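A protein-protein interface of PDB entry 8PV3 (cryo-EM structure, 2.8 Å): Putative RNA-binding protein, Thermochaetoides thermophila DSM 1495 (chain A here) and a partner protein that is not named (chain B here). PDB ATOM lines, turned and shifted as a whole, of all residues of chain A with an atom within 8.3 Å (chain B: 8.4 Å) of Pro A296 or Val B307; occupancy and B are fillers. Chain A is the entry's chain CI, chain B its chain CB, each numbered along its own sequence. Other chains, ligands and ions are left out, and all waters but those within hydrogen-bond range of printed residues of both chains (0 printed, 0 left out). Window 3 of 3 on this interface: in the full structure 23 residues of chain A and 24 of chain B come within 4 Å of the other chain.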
ATOM      1  N   ARG A 291       1.358  24.145  15.783  1.00  0.00           N
ATOM      2  CA  ARG A 291       2.438  25.076  16.094  1.00  0.00           C
ATOM      3  C   ARG A 291       3.541  24.419  16.922  1.00  0.00           C
ATOM      4  O   ARG A 291       4.723  24.665  16.672  1.00  0.00           O
ATOM      5  CB  ARG A 291       1.898  26.327  16.788  1.00  0.00           C
ATOM      6  CG  ARG A 291       2.973  27.396  16.957  1.00  0.00           C
ATOM      7  CD  ARG A 291       2.424  28.789  17.207  1.00  0.00           C
ATOM      8  NE  ARG A 291       1.733  29.307  16.032  1.00  0.00           N
ATOM      9  CZ  ARG A 291       1.326  30.562  15.894  1.00  0.00           C
ATOM     10  NH1 ARG A 291       1.577  31.475  16.817  1.00  0.00           N
ATOM     11  NH2 ARG A 291       0.670  30.913  14.792  1.00  0.00           N
ATOM     12  N   GLN A 292       3.192  23.580  17.908  1.00  0.00           N
ATOM     13  CA  GLN A 292       4.266  22.888  18.630  1.00  0.00           C
ATOM     14  C   GLN A 292       4.924  21.821  17.763  1.00  0.00           C
ATOM     15  O   GLN A 292       6.086  21.465  17.988  1.00  0.00           O
ATOM     16  CB  GLN A 292       3.848  22.249  19.968  1.00  0.00           C
ATOM     17  CG  GLN A 292       3.506  23.179  21.140  1.00  0.00           C
ATOM     18  CD  GLN A 292       2.053  23.550  21.247  1.00  0.00           C
ATOM     19  OE1 GLN A 292       1.192  22.851  20.727  1.00  0.00           O
ATOM     20  NE2 GLN A 292       1.767  24.656  21.924  1.00  0.00           N
ATOM     21  N   LEU A 293       4.199  21.284  16.779  1.00  0.00           N
ATOM     22  CA  LEU A 293       4.835  20.364  15.840  1.00  0.00           C
ATOM     23  C   LEU A 293       5.833  21.092  14.947  1.00  0.00           C
ATOM     24  O   LEU A 293       6.853  20.517  14.548  1.00  0.00           O
ATOM     25  CB  LEU A 293       3.778  19.644  15.005  1.00  0.00           C
ATOM     26  CG  LEU A 293       3.032  18.521  15.727  1.00  0.00           C
ATOM     27  CD1 LEU A 293       2.178  17.740  14.756  1.00  0.00           C
ATOM     28  CD2 LEU A 293       4.003  17.594  16.448  1.00  0.00           C
ATOM     29  N   GLU A 294       5.559  22.355  14.622  1.00  0.00           N
ATOM     30  CA  GLU A 294       6.478  23.167  13.832  1.00  0.00           C
ATOM     31  C   GLU A 294       7.436  23.997  14.682  1.00  0.00           C
ATOM     32  O   GLU A 294       8.235  24.763  14.132  1.00  0.00           O
ATOM     33  CB  GLU A 294       5.698  24.071  12.877  1.00  0.00           C
ATOM     34  CG  GLU A 294       5.321  23.381  11.586  1.00  0.00           C
ATOM     35  CD  GLU A 294       6.532  23.153  10.703  1.00  0.00           C
ATOM     36  OE1 GLU A 294       7.424  24.026  10.684  1.00  0.00           O
ATOM     37  OE2 GLU A 294       6.609  22.094  10.049  1.00  0.00           O
ATOM     38  N   ARG A 295       7.376  23.867  16.006  1.00  0.00           N
ATOM     39  CA  ARG A 295       8.319  24.648  16.800  1.00  0.00           C
ATOM     40  C   ARG A 295       9.693  23.986  16.806  1.00  0.00           C
ATOM     41  O   ARG A 295       9.796  22.772  17.011  1.00  0.00           O
ATOM     42  CB  ARG A 295       7.836  24.803  18.241  1.00  0.00           C
ATOM     43  CG  ARG A 295       6.990  26.038  18.506  1.00  0.00           C
ATOM     44  CD  ARG A 295       6.584  26.109  19.971  1.00  0.00           C
ATOM     45  NE  ARG A 295       5.881  27.346  20.291  1.00  0.00           N
ATOM     46  CZ  ARG A 295       4.560  27.467  20.334  1.00  0.00           C
ATOM     47  NH1 ARG A 295       3.764  26.437  20.102  1.00  0.00           N
ATOM     48  NH2 ARG A 295       4.027  28.650  20.625  1.00  0.00           N
ATOM     49  N   PRO A 296      10.753  24.760  16.584  1.00  0.00           N
ATOM     50  CA  PRO A 296      12.102  24.212  16.746  1.00  0.00           C
ATOM     51  C   PRO A 296      12.419  23.996  18.216  1.00  0.00           C
ATOM     52  O   PRO A 296      12.094  24.823  19.071  1.00  0.00           O
ATOM     53  CB  PRO A 296      12.998  25.289  16.128  1.00  0.00           C
ATOM     54  CG  PRO A 296      12.226  26.551  16.305  1.00  0.00           C
ATOM     55  CD  PRO A 296      10.774  26.173  16.169  1.00  0.00           C
ATOM     56  N   LEU A 297      13.063  22.871  18.505  1.00  0.00           N
ATOM     57  CA  LEU A 297      13.404  22.499  19.868  1.00  0.00           C
ATOM     58  C   LEU A 297      14.909  22.304  19.974  1.00  0.00           C
ATOM     59  O   LEU A 297      15.645  22.458  18.997  1.00  0.00           O
ATOM     60  CB  LEU A 297      12.667  21.225  20.302  1.00  0.00           C
ATOM     61  CG  LEU A 297      11.139  21.300  20.282  1.00  0.00           C
ATOM     62  CD1 LEU A 297      10.528  20.035  20.861  1.00  0.00           C
ATOM     63  CD2 LEU A 297      10.652  22.524  21.042  1.00  0.00           C
ATOM     64  N   SER A 298      15.359  21.960  21.177  1.00  0.00           N
ATOM     65  CA  SER A 298      16.785  21.825  21.424  1.00  0.00           C
ATOM     66  C   SER A 298      17.227  20.366  21.357  1.00  0.00           C
ATOM     67  O   SER A 298      16.439  19.428  21.565  1.00  0.00           O
ATOM     68  CB  SER A 298      17.173  22.428  22.777  1.00  0.00           C
ATOM     69  OG  SER A 298      16.649  21.683  23.859  1.00  0.00           O
ATOM     70  N   GLU A 299      18.529  20.197  21.103  1.00  0.00           N
ATOM     71  CA  GLU A 299      19.075  18.903  20.713  1.00  0.00           C
ATOM     72  C   GLU A 299      18.885  17.848  21.795  1.00  0.00           C
ATOM     73  O   GLU A 299      18.767  16.663  21.479  1.00  0.00           O
ATOM     74  CB  GLU A 299      20.556  19.048  20.349  1.00  0.00           C
ATOM     75  CG  GLU A 299      21.494  19.395  21.501  1.00  0.00           C
ATOM     76  CD  GLU A 299      21.588  20.888  21.769  1.00  0.00           C
ATOM     77  OE1 GLU A 299      20.726  21.649  21.279  1.00  0.00           O
ATOM     78  OE2 GLU A 299      22.537  21.297  22.468  1.00  0.00           O
ATOM     79  N   SER A 300      18.796  18.263  23.066  1.00  0.00           N
ATOM     80  CA  SER A 300      18.616  17.305  24.157  1.00  0.00           C
ATOM     81  C   SER A 300      17.294  16.554  24.029  1.00  0.00           C
ATOM     82  O   SER A 300      17.266  15.315  24.007  1.00  0.00           O
ATOM     83  CB  SER A 300      18.699  18.024  25.501  1.00  0.00           C
ATOM     84  OG  SER A 300      18.525  17.115  26.575  1.00  0.00           O
ATOM     85  N   GLN A 301      16.184  17.285  23.883  1.00  0.00           N
ATOM     86  CA  GLN A 301      14.925  16.592  23.637  1.00  0.00           C
ATOM     87  C   GLN A 301      14.859  16.035  22.222  1.00  0.00           C
ATOM     88  O   GLN A 301      14.005  15.192  21.941  1.00  0.00           O
ATOM     89  CB  GLN A 301      13.712  17.485  23.927  1.00  0.00           C
ATOM     90  CG  GLN A 301      13.620  18.786  23.172  1.00  0.00           C
ATOM     91  CD  GLN A 301      14.178  19.931  23.975  1.00  0.00           C
ATOM     92  OE1 GLN A 301      14.916  19.724  24.938  1.00  0.00           O
ATOM     93  NE2 GLN A 301      13.808  21.150  23.607  1.00  0.00           N
ATOM     94  N   TRP A 302      15.767  16.443  21.331  1.00  0.00           N
ATOM     95  CA  TRP A 302      15.880  15.714  20.065  1.00  0.00           C
ATOM     96  C   TRP A 302      16.428  14.292  20.267  1.00  0.00           C
ATOM     97  O   TRP A 302      15.895  13.333  19.686  1.00  0.00           O
ATOM     98  CB  TRP A 302      16.705  16.521  19.063  1.00  0.00           C
ATOM     99  CG  TRP A 302      15.913  17.635  18.417  1.00  0.00           C
ATOM    100  CD1 TRP A 302      15.179  18.593  19.055  1.00  0.00           C
ATOM    101  CD2 TRP A 302      15.840  17.948  17.021  1.00  0.00           C
ATOM    102  NE1 TRP A 302      14.625  19.456  18.146  1.00  0.00           N
ATOM    103  CE2 TRP A 302      15.017  19.085  16.890  1.00  0.00           C
ATOM    104  CE3 TRP A 302      16.376  17.368  15.868  1.00  0.00           C
ATOM    105  CZ2 TRP A 302      14.719  19.654  15.655  1.00  0.00           C
ATOM    106  CZ3 TRP A 302      16.077  17.937  14.641  1.00  0.00           C
ATOM    107  CH2 TRP A 302      15.257  19.067  14.546  1.00  0.00           C
ATOM    108  N   PRO A 335      21.211  14.127  15.938  1.00  0.00           N
ATOM    109  CA  PRO A 335      21.704  15.425  15.475  1.00  0.00           C
ATOM    110  C   PRO A 335      22.832  15.967  16.351  1.00  0.00           C
ATOM    111  O   PRO A 335      22.800  17.137  16.734  1.00  0.00           O
ATOM    112  CB  PRO A 335      20.467  16.317  15.567  1.00  0.00           C
ATOM    113  CG  PRO A 335      19.684  15.726  16.675  1.00  0.00           C
ATOM    114  CD  PRO A 335      19.873  14.238  16.543  1.00  0.00           C
ATOM    115  N   ASP B 302      13.429  20.401   8.089  1.00  0.00           N
ATOM    116  CA  ASP B 302      14.644  21.020   7.581  1.00  0.00           C
ATOM    117  C   ASP B 302      15.603  21.215   8.748  1.00  0.00           C
ATOM    118  O   ASP B 302      15.261  20.971   9.908  1.00  0.00           O
ATOM    119  CB  ASP B 302      14.337  22.344   6.874  1.00  0.00           C
ATOM    120  CG  ASP B 302      13.599  23.329   7.760  1.00  0.00           C
ATOM    121  OD1 ASP B 302      12.977  22.910   8.762  1.00  0.00           O
ATOM    122  OD2 ASP B 302      13.648  24.535   7.442  1.00  0.00           O
ATOM    123  N   GLU B 303      16.816  21.671   8.427  1.00  0.00           N
ATOM    124  CA  GLU B 303      17.848  21.865   9.437  1.00  0.00           C
ATOM    125  C   GLU B 303      17.631  23.117  10.278  1.00  0.00           C
ATOM    126  O   GLU B 303      18.327  23.298  11.282  1.00  0.00           O
ATOM    127  CB  GLU B 303      19.227  21.919   8.775  1.00  0.00           C
ATOM    128  CG  GLU B 303      19.443  23.125   7.874  1.00  0.00           C
ATOM    129  CD  GLU B 303      19.029  22.866   6.437  1.00  0.00           C
ATOM    130  OE1 GLU B 303      18.296  21.884   6.191  1.00  0.00           O
ATOM    131  OE2 GLU B 303      19.432  23.648   5.552  1.00  0.00           O
ATOM    132  N   SER B 304      16.687  23.982   9.895  1.00  0.00           N
ATOM    133  CA  SER B 304      16.412  25.177  10.684  1.00  0.00           C
ATOM    134  C   SER B 304      15.747  24.838  12.013  1.00  0.00           C
ATOM    135  O   SER B 304      15.790  25.644  12.950  1.00  0.00           O
ATOM    136  CB  SER B 304      15.539  26.144   9.887  1.00  0.00           C
ATOM    137  OG  SER B 304      14.211  25.661   9.787  1.00  0.00           O
ATOM    138  N   LYS B 305      15.122  23.662  12.114  1.00  0.00           N
ATOM    139  CA  LYS B 305      14.524  23.247  13.379  1.00  0.00           C
ATOM    140  C   LYS B 305      15.593  22.891  14.406  1.00  0.00           C
ATOM    141  O   LYS B 305      15.329  22.897  15.615  1.00  0.00           O
ATOM    142  CB  LYS B 305      13.582  22.063  13.153  1.00  0.00           C
ATOM    143  CG  LYS B 305      12.388  22.301  12.208  1.00  0.00           C
ATOM    144  CD  LYS B 305      11.278  23.197  12.785  1.00  0.00           C
ATOM    145  CE  LYS B 305      11.398  24.666  12.377  1.00  0.00           C
ATOM    146  NZ  LYS B 305      10.245  25.474  12.862  1.00  0.00           N
ATOM    147  N   VAL B 306      16.799  22.570  13.946  1.00  0.00           N
ATOM    148  CA  VAL B 306      17.905  22.242  14.841  1.00  0.00           C
ATOM    149  C   VAL B 306      18.394  23.534  15.488  1.00  0.00           C
ATOM    150  O   VAL B 306      18.976  24.393  14.818  1.00  0.00           O
ATOM    151  CB  VAL B 306      19.040  21.531  14.096  1.00  0.00           C
ATOM    152  CG1 VAL B 306      20.154  21.150  15.060  1.00  0.00           C
ATOM    153  CG2 VAL B 306      18.510  20.308  13.368  1.00  0.00           C
ATOM    154  N   VAL B 307      18.161  23.676  16.788  1.00  0.00           N
ATOM    155  CA  VAL B 307      18.586  24.862  17.527  1.00  0.00           C
ATOM    156  C   VAL B 307      19.530  24.435  18.645  1.00  0.00           C
ATOM    157  O   VAL B 307      19.152  23.618  19.496  1.00  0.00           O
ATOM    158  CB  VAL B 307      17.382  25.636  18.086  1.00  0.00           C
ATOM    159  CG1 VAL B 307      17.853  26.773  18.981  1.00  0.00           C
ATOM    160  CG2 VAL B 307      16.523  26.171  16.953  1.00  0.00           C
ATOM    161  N   PRO B 308      20.765  24.955  18.685  1.00  0.00           N
ATOM    162  CA  PRO B 308      21.726  24.599  19.729  1.00  0.00           C
ATOM    163  C   PRO B 308      21.654  25.534  20.932  1.00  0.00           C
ATOM    164  O   PRO B 308      21.351  25.069  22.031  1.00  0.00           O
ATOM    165  CB  PRO B 308      23.079  24.727  19.019  1.00  0.00           C
ATOM    166  CG  PRO B 308      22.810  25.543  17.753  1.00  0.00           C
ATOM    167  CD  PRO B 308      21.348  25.888  17.711  1.00  0.00           C
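OE1 of Glu A294 lies within salt-bridge range of NZ of Lys B305. O of Lys B305 lies close to O of Leu A297, 3.4 Å away. The backbone carbonyl oxygen of Val B307 lies close to the side-chain carboxylate of Glu A299, at 3.1 Å.
The backbone carbonyl oxygen of Leu A297 sits at hydrogen-bond distance from the indole nitrogen of Trp A302 (3.3 Å). The side-chain amide oxygen (OE1) of Gln A301 is in hydrogen-bond range of the side-chain hydroxyl (OG) of Ser A298 (2.8 Å).
Among the printed residues, pairs that only touch across the chains: Pro A296 with Lys B305, Pro A296 with Val B307, Leu A297 with Val B307, Ser A298 with Val B307, Glu A299 with Pro B308, Trp A302 with Lys B305 and Trp A302 with Val B306.
Of the printed residues of chain B, Trp A302 touches Lys B305 (3.3 Å) and Val B306 (3.6 Å). Of the printed residues of chain A, Val B306 touches Trp A302. Val B307 touches four residues of chain A. The nearest residue of chain B that does not touch Pro A296 is Ser B304 (4.2 Å).
Of the 7 printed residues of chain B, 4 touch a printed residue of chain A. Printed residues of chain A that touch a printed residue of chain B: Glu A294, Pro A296, Leu A297, Ser A298, Glu A299 and Trp A302. Hydrophobic or aromatic side chains of chain A that line the printed part of chain B: Pro A296 and Trp A302. Among the printed residues, 10 pairs touch across the chains.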
